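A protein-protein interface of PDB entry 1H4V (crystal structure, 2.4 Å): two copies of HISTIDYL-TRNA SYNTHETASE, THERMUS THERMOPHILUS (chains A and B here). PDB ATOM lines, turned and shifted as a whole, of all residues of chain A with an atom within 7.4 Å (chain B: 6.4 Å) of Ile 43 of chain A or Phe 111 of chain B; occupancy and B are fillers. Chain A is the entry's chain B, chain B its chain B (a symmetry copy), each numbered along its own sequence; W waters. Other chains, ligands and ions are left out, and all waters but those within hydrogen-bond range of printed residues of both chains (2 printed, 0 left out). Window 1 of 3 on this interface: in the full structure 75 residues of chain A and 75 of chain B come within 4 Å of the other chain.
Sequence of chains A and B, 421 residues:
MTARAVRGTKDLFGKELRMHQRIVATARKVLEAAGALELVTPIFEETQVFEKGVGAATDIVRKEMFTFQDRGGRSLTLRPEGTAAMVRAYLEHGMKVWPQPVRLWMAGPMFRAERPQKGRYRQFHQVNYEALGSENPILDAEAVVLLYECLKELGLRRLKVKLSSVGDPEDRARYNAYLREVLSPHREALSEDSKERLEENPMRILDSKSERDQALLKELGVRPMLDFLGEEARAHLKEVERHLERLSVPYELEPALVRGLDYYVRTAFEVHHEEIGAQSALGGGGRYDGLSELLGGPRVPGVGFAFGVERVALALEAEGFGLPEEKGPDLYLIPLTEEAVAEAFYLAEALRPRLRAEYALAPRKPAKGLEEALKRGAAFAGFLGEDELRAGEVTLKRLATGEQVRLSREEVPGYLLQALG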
ATOM      1  N   VAL A  40     -15.983  -9.767  -0.142  1.00  0.00           N
ATOM      2  CA  VAL A  40     -16.262  -9.430   1.253  1.00  0.00           C
ATOM      3  C   VAL A  40     -15.602 -10.488   2.147  1.00  0.00           C
ATOM      4  O   VAL A  40     -15.972 -11.662   2.096  1.00  0.00           O
ATOM      5  CB  VAL A  40     -17.784  -9.406   1.575  1.00  0.00           C
ATOM      6  CG1 VAL A  40     -17.977  -9.038   3.045  1.00  0.00           C
ATOM      7  CG2 VAL A  40     -18.519  -8.398   0.682  1.00  0.00           C
ATOM      8  N   THR A  41     -14.619 -10.085   2.948  1.00  0.00           N
ATOM      9  CA  THR A  41     -13.958 -11.032   3.838  1.00  0.00           C
ATOM     10  C   THR A  41     -14.611 -10.980   5.207  1.00  0.00           C
ATOM     11  O   THR A  41     -15.412 -10.084   5.489  1.00  0.00           O
ATOM     12  CB  THR A  41     -12.460 -10.718   4.003  1.00  0.00           C
ATOM     13  OG1 THR A  41     -12.297  -9.444   4.642  1.00  0.00           O
ATOM     14  CG2 THR A  41     -11.781 -10.690   2.655  1.00  0.00           C
ATOM     15  N   PRO A  42     -14.284 -11.945   6.081  1.00  0.00           N
ATOM     16  CA  PRO A  42     -14.879 -11.951   7.420  1.00  0.00           C
ATOM     17  C   PRO A  42     -14.423 -10.790   8.299  1.00  0.00           C
ATOM     18  O   PRO A  42     -13.381 -10.178   8.064  1.00  0.00           O
ATOM     19  CB  PRO A  42     -14.441 -13.303   7.981  1.00  0.00           C
ATOM     20  CG  PRO A  42     -14.386 -14.163   6.759  1.00  0.00           C
ATOM     21  CD  PRO A  42     -13.664 -13.251   5.790  1.00  0.00           C
ATOM     22  N   ILE A  43     -15.225 -10.489   9.313  1.00  0.00           N
ATOM     23  CA  ILE A  43     -14.911  -9.421  10.249  1.00  0.00           C
ATOM     24  C   ILE A  43     -13.656  -9.769  11.067  1.00  0.00           C
ATOM     25  O   ILE A  43     -12.892  -8.891  11.450  1.00  0.00           O
ATOM     26  CB  ILE A  43     -16.099  -9.180  11.195  1.00  0.00           C
ATOM     27  CG1 ILE A  43     -17.305  -8.659  10.393  1.00  0.00           C
ATOM     28  CG2 ILE A  43     -15.697  -8.244  12.305  1.00  0.00           C
ATOM     29  CD1 ILE A  43     -17.127  -7.281   9.755  1.00  0.00           C
ATOM     30  N   PHE A  44     -13.451 -11.051  11.346  1.00  0.00           N
ATOM     31  CA  PHE A  44     -12.268 -11.474  12.094  1.00  0.00           C
ATOM     32  C   PHE A  44     -11.578 -12.642  11.411  1.00  0.00           C
ATOM     33  O   PHE A  44     -12.188 -13.368  10.623  1.00  0.00           O
ATOM     34  CB  PHE A  44     -12.618 -11.843  13.548  1.00  0.00           C
ATOM     35  CG  PHE A  44     -13.654 -12.932  13.692  1.00  0.00           C
ATOM     36  CD1 PHE A  44     -13.387 -14.235  13.287  1.00  0.00           C
ATOM     37  CD2 PHE A  44     -14.891 -12.652  14.265  1.00  0.00           C
ATOM     38  CE1 PHE A  44     -14.339 -15.253  13.451  1.00  0.00           C
ATOM     39  CE2 PHE A  44     -15.851 -13.660  14.435  1.00  0.00           C
ATOM     40  CZ  PHE A  44     -15.571 -14.965  14.024  1.00  0.00           C
ATOM     41  N   GLU A  45     -10.297 -12.809  11.715  1.00  0.00           N
ATOM     42  CA  GLU A  45      -9.488 -13.883  11.140  1.00  0.00           C
ATOM     43  C   GLU A  45      -8.427 -14.327  12.131  1.00  0.00           C
ATOM     44  O   GLU A  45      -8.291 -13.753  13.222  1.00  0.00           O
ATOM     45  CB  GLU A  45      -8.792 -13.395   9.866  1.00  0.00           C
ATOM     46  CG  GLU A  45      -9.741 -12.794   8.872  1.00  0.00           C
ATOM     47  CD  GLU A  45      -9.391 -13.131   7.446  1.00  0.00           C
ATOM     48  OE1 GLU A  45      -8.756 -14.182   7.216  1.00  0.00           O
ATOM     49  OE2 GLU A  45      -9.775 -12.352   6.554  1.00  0.00           O
ATOM     50  N   PHE A  50      -2.800 -11.059  10.116  1.00  0.00           N
ATOM     51  CA  PHE A  50      -2.455  -9.653  10.258  1.00  0.00           C
ATOM     52  C   PHE A  50      -1.129  -9.289  10.903  1.00  0.00           C
ATOM     53  O   PHE A  50      -0.845  -8.104  11.072  1.00  0.00           O
ATOM     54  CB  PHE A  50      -3.607  -8.936  10.971  1.00  0.00           C
ATOM     55  CG  PHE A  50      -4.918  -9.045  10.238  1.00  0.00           C
ATOM     56  CD1 PHE A  50      -6.000  -9.706  10.806  1.00  0.00           C
ATOM     57  CD2 PHE A  50      -5.057  -8.510   8.960  1.00  0.00           C
ATOM     58  CE1 PHE A  50      -7.199  -9.832  10.112  1.00  0.00           C
ATOM     59  CE2 PHE A  50      -6.247  -8.634   8.265  1.00  0.00           C
ATOM     60  CZ  PHE A  50      -7.321  -9.293   8.836  1.00  0.00           C
ATOM     61  N   PHE A  68      -8.362 -11.835  20.341  1.00  0.00           N
ATOM     62  CA  PHE A  68      -9.004 -12.653  21.356  1.00  0.00           C
ATOM     63  C   PHE A  68      -9.028 -14.087  20.871  1.00  0.00           C
ATOM     64  O   PHE A  68      -8.849 -14.345  19.687  1.00  0.00           O
ATOM     65  CB  PHE A  68     -10.430 -12.152  21.612  1.00  0.00           C
ATOM     66  CG  PHE A  68     -11.331 -12.232  20.408  1.00  0.00           C
ATOM     67  CD1 PHE A  68     -12.109 -13.363  20.178  1.00  0.00           C
ATOM     68  CD2 PHE A  68     -11.377 -11.189  19.488  1.00  0.00           C
ATOM     69  CE1 PHE A  68     -12.921 -13.458  19.039  1.00  0.00           C
ATOM     70  CE2 PHE A  68     -12.181 -11.266  18.348  1.00  0.00           C
ATOM     71  CZ  PHE A  68     -12.957 -12.407  18.122  1.00  0.00           C
ATOM     72  N   THR A  77      -8.454 -12.238  15.453  1.00  0.00           N
ATOM     73  CA  THR A  77      -8.294 -10.786  15.430  1.00  0.00           C
ATOM     74  C   THR A  77      -9.310 -10.073  14.534  1.00  0.00           C
ATOM     75  O   THR A  77      -9.594 -10.506  13.421  1.00  0.00           O
ATOM     76  CB  THR A  77      -6.847 -10.394  14.982  1.00  0.00           C
ATOM     77  OG1 THR A  77      -5.916 -10.680  16.040  1.00  0.00           O
ATOM     78  CG2 THR A  77      -6.766  -8.917  14.635  1.00  0.00           C
ATOM     79  N   LEU A  78      -9.863  -8.980  15.041  1.00  0.00           N
ATOM     80  CA  LEU A  78     -10.819  -8.168  14.294  1.00  0.00           C
ATOM     81  C   LEU A  78     -10.044  -7.488  13.164  1.00  0.00           C
ATOM     82  O   LEU A  78      -8.997  -6.894  13.399  1.00  0.00           O
ATOM     83  CB  LEU A  78     -11.441  -7.115  15.218  1.00  0.00           C
ATOM     84  CG  LEU A  78     -12.875  -7.314  15.720  1.00  0.00           C
ATOM     85  CD1 LEU A  78     -13.115  -8.744  16.113  1.00  0.00           C
ATOM     86  CD2 LEU A  78     -13.129  -6.396  16.894  1.00  0.00           C
ATOM     87  N   ARG A  79     -10.557  -7.595  11.943  1.00  0.00           N
ATOM     88  CA  ARG A  79      -9.915  -7.007  10.772  1.00  0.00           C
ATOM     89  C   ARG A  79      -9.440  -5.555  10.966  1.00  0.00           C
ATOM     90  O   ARG A  79     -10.250  -4.647  11.149  1.00  0.00           O
ATOM     91  CB  ARG A  79     -10.873  -7.061   9.584  1.00  0.00           C
ATOM     92  CG  ARG A  79     -10.270  -6.564   8.295  1.00  0.00           C
ATOM     93  CD  ARG A  79     -11.357  -6.003   7.402  1.00  0.00           C
ATOM     94  NE  ARG A  79     -12.257  -7.039   6.932  1.00  0.00           N
ATOM     95  CZ  ARG A  79     -13.552  -6.858   6.727  1.00  0.00           C
ATOM     96  NH1 ARG A  79     -14.098  -5.678   6.967  1.00  0.00           N
ATOM     97  NH2 ARG A  79     -14.291  -7.850   6.257  1.00  0.00           N
ATOM     98  N   PRO A  80      -8.112  -5.327  10.921  1.00  0.00           N
ATOM     99  CA  PRO A  80      -7.508  -3.998  11.085  1.00  0.00           C
ATOM    100  C   PRO A  80      -7.156  -3.330   9.752  1.00  0.00           C
ATOM    101  O   PRO A  80      -6.937  -2.122   9.690  1.00  0.00           O
ATOM    102  CB  PRO A  80      -6.256  -4.301  11.887  1.00  0.00           C
ATOM    103  CG  PRO A  80      -5.802  -5.560  11.239  1.00  0.00           C
ATOM    104  CD  PRO A  80      -7.086  -6.375  11.080  1.00  0.00           C
ATOM    105  N   GLY A 108     -15.787  -2.016   3.784  1.00  0.00           N
ATOM    106  CA  GLY A 108     -16.258  -2.596   5.025  1.00  0.00           C
ATOM    107  C   GLY A 108     -15.617  -2.005   6.257  1.00  0.00           C
ATOM    108  O   GLY A 108     -14.743  -1.158   6.160  1.00  0.00           O
ATOM    109  N   PRO A 109     -16.043  -2.434   7.444  1.00  0.00           N
ATOM    110  CA  PRO A 109     -15.461  -1.901   8.677  1.00  0.00           C
ATOM    111  C   PRO A 109     -14.069  -2.440   9.004  1.00  0.00           C
ATOM    112  O   PRO A 109     -13.730  -3.565   8.636  1.00  0.00           O
ATOM    113  CB  PRO A 109     -16.493  -2.294   9.730  1.00  0.00           C
ATOM    114  CG  PRO A 109     -17.016  -3.569   9.211  1.00  0.00           C
ATOM    115  CD  PRO A 109     -17.227  -3.257   7.742  1.00  0.00           C
ATOM    116  N   MET A 110     -13.273  -1.608   9.672  1.00  0.00           N
ATOM    117  CA  MET A 110     -11.936  -1.961  10.122  1.00  0.00           C
ATOM    118  C   MET A 110     -11.933  -1.602  11.606  1.00  0.00           C
ATOM    119  O   MET A 110     -12.730  -0.784  12.070  1.00  0.00           O
ATOM    120  CB  MET A 110     -10.850  -1.150   9.425  1.00  0.00           C
ATOM    121  CG  MET A 110     -10.787  -1.329   7.934  1.00  0.00           C
ATOM    122  SD  MET A 110     -10.353  -2.993   7.445  1.00  0.00           S
ATOM    123  CE  MET A 110     -10.798  -2.990   5.651  1.00  0.00           C
ATOM    124  N   PHE A 111     -11.019  -2.211  12.342  1.00  0.00           N
ATOM    125  CA  PHE A 111     -10.950  -2.022  13.778  1.00  0.00           C
ATOM    126  C   PHE A 111      -9.551  -1.674  14.226  1.00  0.00           C
ATOM    127  O   PHE A 111      -8.582  -2.347  13.903  1.00  0.00           O
ATOM    128  CB  PHE A 111     -11.489  -3.292  14.423  1.00  0.00           C
ATOM    129  CG  PHE A 111     -12.867  -3.629  13.954  1.00  0.00           C
ATOM    130  CD1 PHE A 111     -13.975  -3.010  14.532  1.00  0.00           C
ATOM    131  CD2 PHE A 111     -13.060  -4.487  12.876  1.00  0.00           C
ATOM    132  CE1 PHE A 111     -15.264  -3.243  14.044  1.00  0.00           C
ATOM    133  CE2 PHE A 111     -14.339  -4.729  12.374  1.00  0.00           C
ATOM    134  CZ  PHE A 111     -15.445  -4.104  12.958  1.00  0.00           C
ATOM    135  N   GLN A 123     -13.692   2.065  15.161  1.00  0.00           N
ATOM    136  CA  GLN A 123     -14.339   1.314  14.087  1.00  0.00           C
ATOM    137  C   GLN A 123     -14.520   2.329  12.972  1.00  0.00           C
ATOM    138  O   GLN A 123     -15.203   3.338  13.150  1.00  0.00           O
ATOM    139  CB  GLN A 123     -15.726   0.741  14.435  1.00  0.00           C
ATOM    140  CG  GLN A 123     -16.291  -0.056  13.226  1.00  0.00           C
ATOM    141  CD  GLN A 123     -17.662  -0.712  13.425  1.00  0.00           C
ATOM    142  OE1 GLN A 123     -17.940  -1.319  14.455  1.00  0.00           O
ATOM    143  NE2 GLN A 123     -18.510  -0.617  12.408  1.00  0.00           N
ATOM    144  N   THR B   9     -16.923 -19.059   9.070  1.00  0.00           N
ATOM    145  CA  THR B   9     -16.877 -17.794   8.342  1.00  0.00           C
ATOM    146  C   THR B   9     -16.453 -18.081   6.907  1.00  0.00           C
ATOM    147  O   THR B   9     -15.922 -19.146   6.615  1.00  0.00           O
ATOM    148  CB  THR B   9     -15.860 -16.823   8.960  1.00  0.00           C
ATOM    149  OG1 THR B   9     -14.526 -17.249   8.636  1.00  0.00           O
ATOM    150  CG2 THR B   9     -16.032 -16.774  10.474  1.00  0.00           C
ATOM    151  N   ILE B  43     -20.205  -3.115  15.119  1.00  0.00           N
ATOM    152  CA  ILE B  43     -19.960  -4.548  15.127  1.00  0.00           C
ATOM    153  C   ILE B  43     -19.875  -5.076  16.569  1.00  0.00           C
ATOM    154  O   ILE B  43     -20.247  -6.210  16.847  1.00  0.00           O
ATOM    155  CB  ILE B  43     -18.654  -4.866  14.378  1.00  0.00           C
ATOM    156  CG1 ILE B  43     -18.805  -4.501  12.891  1.00  0.00           C
ATOM    157  CG2 ILE B  43     -18.278  -6.310  14.583  1.00  0.00           C
ATOM    158  CD1 ILE B  43     -19.825  -5.329  12.109  1.00  0.00           C
ATOM    159  N   GLU B  64     -21.661 -18.683  24.227  1.00  0.00           N
ATOM    160  CA  GLU B  64     -21.969 -18.542  22.817  1.00  0.00           C
ATOM    161  C   GLU B  64     -21.898 -17.119  22.259  1.00  0.00           C
ATOM    162  O   GLU B  64     -22.570 -16.799  21.286  1.00  0.00           O
ATOM    163  CB  GLU B  64     -23.343 -19.157  22.540  1.00  0.00           C
ATOM    164  CG  GLU B  64     -23.366 -20.671  22.737  1.00  0.00           C
ATOM    165  CD  GLU B  64     -24.254 -21.369  21.721  1.00  0.00           C
ATOM    166  OE1 GLU B  64     -25.487 -21.163  21.771  1.00  0.00           O
ATOM    167  OE2 GLU B  64     -23.711 -22.110  20.867  1.00  0.00           O
ATOM    168  N   MET B  65     -21.071 -16.276  22.867  1.00  0.00           N
ATOM    169  CA  MET B  65     -20.887 -14.895  22.420  1.00  0.00           C
ATOM    170  C   MET B  65     -19.401 -14.537  22.447  1.00  0.00           C
ATOM    171  O   MET B  65     -18.700 -14.864  23.403  1.00  0.00           O
ATOM    172  CB  MET B  65     -21.640 -13.923  23.335  1.00  0.00           C
ATOM    173  CG  MET B  65     -23.096 -13.670  22.972  1.00  0.00           C
ATOM    174  SD  MET B  65     -23.939 -12.610  24.200  1.00  0.00           S
ATOM    175  CE  MET B  65     -22.631 -11.543  24.725  1.00  0.00           C
ATOM    176  N   PHE B  66     -18.916 -13.878  21.400  1.00  0.00           N
ATOM    177  CA  PHE B  66     -17.517 -13.482  21.368  1.00  0.00           C
ATOM    178  C   PHE B  66     -17.387 -12.229  22.219  1.00  0.00           C
ATOM    179  O   PHE B  66     -17.857 -11.160  21.845  1.00  0.00           O
ATOM    180  CB  PHE B  66     -17.044 -13.185  19.941  1.00  0.00           C
ATOM    181  CG  PHE B  66     -17.009 -14.385  19.039  1.00  0.00           C
ATOM    182  CD1 PHE B  66     -18.040 -14.626  18.141  1.00  0.00           C
ATOM    183  CD2 PHE B  66     -15.928 -15.259  19.067  1.00  0.00           C
ATOM    184  CE1 PHE B  66     -17.994 -15.720  17.273  1.00  0.00           C
ATOM    185  CE2 PHE B  66     -15.871 -16.360  18.204  1.00  0.00           C
ATOM    186  CZ  PHE B  66     -16.904 -16.590  17.306  1.00  0.00           C
ATOM    187  N   LEU B  78     -18.996  -8.916  20.478  1.00  0.00           N
ATOM    188  CA  LEU B  78     -19.325  -8.888  19.056  1.00  0.00           C
ATOM    189  C   LEU B  78     -20.838  -9.086  18.942  1.00  0.00           C
ATOM    190  O   LEU B  78     -21.391 -10.004  19.541  1.00  0.00           O
ATOM    191  CB  LEU B  78     -18.587 -10.017  18.330  1.00  0.00           C
ATOM    192  CG  LEU B  78     -17.367  -9.679  17.467  1.00  0.00           C
ATOM    193  CD1 LEU B  78     -16.492  -8.664  18.145  1.00  0.00           C
ATOM    194  CD2 LEU B  78     -16.585 -10.941  17.182  1.00  0.00           C
ATOM    195  N   ARG B  79     -21.496  -8.215  18.186  1.00  0.00           N
ATOM    196  CA  ARG B  79     -22.942  -8.277  18.001  1.00  0.00           C
ATOM    197  C   ARG B  79     -23.486  -9.685  17.692  1.00  0.00           C
ATOM    198  O   ARG B  79     -23.187 -10.258  16.644  1.00  0.00           O
ATOM    199  CB  ARG B  79     -23.354  -7.328  16.877  1.00  0.00           C
ATOM    200  CG  ARG B  79     -24.845  -7.246  16.669  1.00  0.00           C
ATOM    201  CD  ARG B  79     -25.143  -6.902  15.224  1.00  0.00           C
ATOM    202  NE  ARG B  79     -24.719  -5.555  14.892  1.00  0.00           N
ATOM    203  CZ  ARG B  79     -24.247  -5.199  13.707  1.00  0.00           C
ATOM    204  NH1 ARG B  79     -24.128  -6.100  12.748  1.00  0.00           N
ATOM    205  NH2 ARG B  79     -23.921  -3.937  13.480  1.00  0.00           N
ATOM    206  N   PRO B  80     -24.297 -10.250  18.607  1.00  0.00           N
ATOM    207  CA  PRO B  80     -24.896 -11.583  18.454  1.00  0.00           C
ATOM    208  C   PRO B  80     -26.339 -11.538  17.945  1.00  0.00           C
ATOM    209  O   PRO B  80     -26.874 -12.540  17.473  1.00  0.00           O
ATOM    210  CB  PRO B  80     -24.836 -12.137  19.865  1.00  0.00           C
ATOM    211  CG  PRO B  80     -25.204 -10.934  20.658  1.00  0.00           C
ATOM    212  CD  PRO B  80     -24.397  -9.807  20.011  1.00  0.00           C
ATOM    213  N   GLU B  81     -26.964 -10.372  18.063  1.00  0.00           N
ATOM    214  CA  GLU B  81     -28.353 -10.173  17.643  1.00  0.00           C
ATOM    215  C   GLU B  81     -28.523  -8.712  17.254  1.00  0.00           C
ATOM    216  O   GLU B  81     -27.664  -7.885  17.538  1.00  0.00           O
ATOM    217  CB  GLU B  81     -29.317 -10.481  18.795  1.00  0.00           C
ATOM    218  CG  GLU B  81     -29.163  -9.518  19.966  1.00  0.00           C
ATOM    219  CD  GLU B  81     -30.387  -9.477  20.863  1.00  0.00           C
ATOM    220  OE1 GLU B  81     -30.768 -10.541  21.400  1.00  0.00           O
ATOM    221  OE2 GLU B  81     -30.972  -8.381  21.030  1.00  0.00           O
ATOM    222  N   PRO B 109     -23.708  -8.348   9.698  1.00  0.00           N
ATOM    223  CA  PRO B 109     -23.207  -9.589  10.291  1.00  0.00           C
ATOM    224  C   PRO B 109     -23.525  -9.751  11.778  1.00  0.00           C
ATOM    225  O   PRO B 109     -23.651  -8.765  12.503  1.00  0.00           O
ATOM    226  CB  PRO B 109     -21.705  -9.502  10.030  1.00  0.00           C
ATOM    227  CG  PRO B 109     -21.448  -8.054  10.102  1.00  0.00           C
ATOM    228  CD  PRO B 109     -22.591  -7.482   9.285  1.00  0.00           C
ATOM    229  N   MET B 110     -23.674 -11.005  12.199  1.00  0.00           N
ATOM    230  CA  MET B 110     -23.923 -11.364  13.587  1.00  0.00           C
ATOM    231  C   MET B 110     -22.862 -12.417  13.897  1.00  0.00           C
ATOM    232  O   MET B 110     -22.321 -13.067  13.000  1.00  0.00           O
ATOM    233  CB  MET B 110     -25.299 -11.985  13.794  1.00  0.00           C
ATOM    234  CG  MET B 110     -26.455 -11.092  13.441  1.00  0.00           C
ATOM    235  SD  MET B 110     -26.563  -9.641  14.479  1.00  0.00           S
ATOM    236  CE  MET B 110     -27.744  -8.582  13.529  1.00  0.00           C
ATOM    237  N   PHE B 111     -22.581 -12.588  15.177  1.00  0.00           N
ATOM    238  CA  PHE B 111     -21.541 -13.501  15.612  1.00  0.00           C
ATOM    239  C   PHE B 111     -22.039 -14.439  16.686  1.00  0.00           C
ATOM    240  O   PHE B 111     -22.604 -14.029  17.691  1.00  0.00           O
ATOM    241  CB  PHE B 111     -20.357 -12.653  16.055  1.00  0.00           C
ATOM    242  CG  PHE B 111     -19.891 -11.720  14.985  1.00  0.00           C
ATOM    243  CD1 PHE B 111     -19.035 -12.174  13.983  1.00  0.00           C
ATOM    244  CD2 PHE B 111     -20.378 -10.419  14.917  1.00  0.00           C
ATOM    245  CE1 PHE B 111     -18.663 -11.343  12.923  1.00  0.00           C
ATOM    246  CE2 PHE B 111     -20.019  -9.575  13.865  1.00  0.00           C
ATOM    247  CZ  PHE B 111     -19.161 -10.038  12.863  1.00  0.00           C
ATOM    248  N   ARG B 112     -21.803 -15.715  16.431  1.00  0.00           N
ATOM    249  CA  ARG B 112     -22.231 -16.832  17.273  1.00  0.00           C
ATOM    250  C   ARG B 112     -20.959 -17.645  17.535  1.00  0.00           C
ATOM    251  O   ARG B 112     -20.249 -17.997  16.605  1.00  0.00           O
ATOM    252  CB  ARG B 112     -23.229 -17.671  16.464  1.00  0.00           C
ATOM    253  CG  ARG B 112     -24.116 -18.628  17.235  1.00  0.00           C
ATOM    254  CD  ARG B 112     -25.315 -19.031  16.355  1.00  0.00           C
ATOM    255  NE  ARG B 112     -24.920 -19.873  15.220  1.00  0.00           N
ATOM    256  CZ  ARG B 112     -25.633 -19.988  14.094  1.00  0.00           C
ATOM    257  NH1 ARG B 112     -26.770 -19.309  13.939  1.00  0.00           N
ATOM    258  NH2 ARG B 112     -25.246 -20.797  13.117  1.00  0.00           N
ATOM    259  N   ALA B 113     -20.665 -17.943  18.790  1.00  0.00           N
ATOM    260  CA  ALA B 113     -19.460 -18.699  19.096  1.00  0.00           C
ATOM    261  C   ALA B 113     -19.711 -20.202  19.305  1.00  0.00           C
ATOM    262  O   ALA B 113     -19.822 -20.673  20.428  1.00  0.00           O
ATOM    263  CB  ALA B 113     -18.789 -18.107  20.311  1.00  0.00           C
ATOM    264  N   ARG B 122     -20.494 -19.154  12.234  1.00  0.00           N
ATOM    265  CA  ARG B 122     -20.139 -18.426  13.445  1.00  0.00           C
ATOM    266  C   ARG B 122     -20.311 -16.954  13.094  1.00  0.00           C
ATOM    267  O   ARG B 122     -20.504 -16.116  13.972  1.00  0.00           O
ATOM    268  CB  ARG B 122     -18.718 -18.769  13.890  1.00  0.00           C
ATOM    269  CG  ARG B 122     -18.637 -20.144  14.556  1.00  0.00           C
ATOM    270  CD  ARG B 122     -17.212 -20.671  14.601  1.00  0.00           C
ATOM    271  NE  ARG B 122     -16.483 -20.238  15.784  1.00  0.00           N
ATOM    272  CZ  ARG B 122     -15.158 -20.233  15.874  1.00  0.00           C
ATOM    273  NH1 ARG B 122     -14.420 -20.631  14.840  1.00  0.00           N
ATOM    274  NH2 ARG B 122     -14.568 -19.849  17.001  1.00  0.00           N
ATOM    275  N   GLN B 123     -20.240 -16.647  11.798  1.00  0.00           N
ATOM    276  CA  GLN B 123     -20.515 -15.295  11.318  1.00  0.00           C
ATOM    277  C   GLN B 123     -21.608 -15.477  10.281  1.00  0.00           C
ATOM    278  O   GLN B 123     -21.413 -16.168   9.281  1.00  0.00           O
ATOM    279  CB  GLN B 123     -19.326 -14.592  10.634  1.00  0.00           C
ATOM    280  CG  GLN B 123     -19.737 -13.157  10.197  1.00  0.00           C
ATOM    281  CD  GLN B 123     -18.650 -12.316   9.519  1.00  0.00           C
ATOM    282  OE1 GLN B 123     -17.503 -12.276   9.954  1.00  0.00           O
ATOM    283  NE2 GLN B 123     -19.031 -11.608   8.462  1.00  0.00           N
ATOM    284  N   PHE B 124     -22.775 -14.899  10.533  1.00  0.00           N
ATOM    285  CA  PHE B 124     -23.858 -14.990   9.568  1.00  0.00           C
ATOM    286  C   PHE B 124     -24.404 -13.591   9.402  1.00  0.00           C
ATOM    287  O   PHE B 124     -23.962 -12.671  10.085  1.00  0.00           O
ATOM    288  CB  PHE B 124     -24.951 -15.966  10.039  1.00  0.00           C
ATOM    289  CG  PHE B 124     -25.490 -15.680  11.430  1.00  0.00           C
ATOM    290  CD1 PHE B 124     -26.705 -15.029  11.598  1.00  0.00           C
ATOM    291  CD2 PHE B 124     -24.786 -16.088  12.565  1.00  0.00           C
ATOM    292  CE1 PHE B 124     -27.225 -14.790  12.868  1.00  0.00           C
ATOM    293  CE2 PHE B 124     -25.290 -15.852  13.847  1.00  0.00           C
ATOM    294  CZ  PHE B 124     -26.516 -15.200  13.996  1.00  0.00           C
HETATM  295  O   HOH W   1     -17.518  -9.545   6.627  1.00  0.00           O
HETATM  296  O   HOH W   2     -12.154 -15.852   8.963  1.00  0.00           O
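The backbone NH (N) of Ile 43 of chain A sits at hydrogen-bond distance from the side-chain amide oxygen (OE1) of Gln 123 of chain B (3.0 Å). N of Ile 43 of chain B sits at hydrogen-bond distance from OE1 of Gln 123 of chain A (3.0 Å).
O of Ile 43 of chain B is in hydrogen-bond range of N of Arg 79 of chain B (2.7 Å). The backbone carbonyl oxygen (O) of Phe 66 of chain B lies within hydrogen-bond range of the backbone NH (N) of Leu 78 of chain B (2.9 Å). The backbone carbonyl oxygen (O) of Arg 79 of chain A sits at hydrogen-bond distance from the backbone NH (N) of Phe 111 of chain A. O of Arg 79 of chain B sits at hydrogen-bond distance from N of Phe 111 of chain B (2.8 Å).
Pro 42 of chain A touches Gln 123 of chain B. Ile 43 of chain A touches Ile 43 of chain B (CG2 to CG2, 3.9 Å). CG1 of Ile 43 of chain A touches CZ of Phe 111 of chain B, 3.4 Å away. Phe 44 of chain A touches Thr 9 of chain B. Phe 66 of chain B touches Phe 44 of chain A. Phe 111 of chain B touches Phe 44 of chain A (CD1 to CE2, 3.5 Å). Phe 66 of chain B touches Phe 68 of chain A (CD2 to CE1, 3.5 Å). CD1 of Leu 78 of chain A touches CD1 of Leu 78 of chain B (3.9 Å).
Of the printed residues of chain B, Ile 43 of chain A touches Ile 43, Phe 111 and Gln 123. Of the printed residues of chain B, Phe 44 of chain A touches Thr 9, Phe 66, Leu 78 and Phe 111. Of the printed residues of chain B, Phe 68 of chain A touches Phe 66 (3.5 Å). Thr 77 of chain A touches none of the printed residues of chain B. Of the printed residues of chain B, Gln 123 of chain A touches Ile 43 (3.0 Å). Printed residues of chain A within 4 Å of Thr 9 of chain B: Pro 42 (3.6 Å) and Phe 44 (3.7 Å). Phe 111 of chain B touches just these residues of chain A: Ile 43 (3.4 Å) and Phe 44 (3.5 Å). The nearest residue of chain B that does not touch Ile 43 of chain A is Pro 109 of chain B (4.2 Å). The nearest residue of chain A that does not touch Phe 111 of chain B is Pro 42 of chain A (6.3 Å).
Of the 17 printed residues of chain B, 6 touch a printed residue of chain A. Printed residues of chain B that touch a printed residue of chain A: Thr 9, Ile 43, Phe 66, Leu 78, Phe 111 and Gln 123. Hydrophobic or aromatic side chains of chain B that line the printed part of chain A: Ile 43, Phe 66, Leu 78 and Phe 111. Of the 17 printed residues of chain A, 7 touch a printed residue of chain B.
Ile 43 of chain A touches Phe 111 of chain B, and with the chains exchanged Phe 111 of chain A touches Ile 43 of chain B. Ile 43 of chain A touches Gln 123 of chain B, and with the chains exchanged Gln 123 of chain A touches Ile 43 of chain B. Leu 78 of chain B touches its own counterpart, Leu 78 of chain A. 8 positions are printed for both chains. Of the 13 pairs that touch across the chains among the printed residues, 6 have their exchanged pair printed and touching as well.
Water W1 bridges the backbone carbonyl oxygen (O) of Thr 41 of chain A and the side-chain amide nitrogen (NE2) of Gln 123 of chain B. Water W2 lies within hydrogen-bond range of the side-chain hydroxyl of Thr 9 of chain B (2.8 Å) and the backbone carbonyl oxygen of Phe 44 of chain A (3.0 Å).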
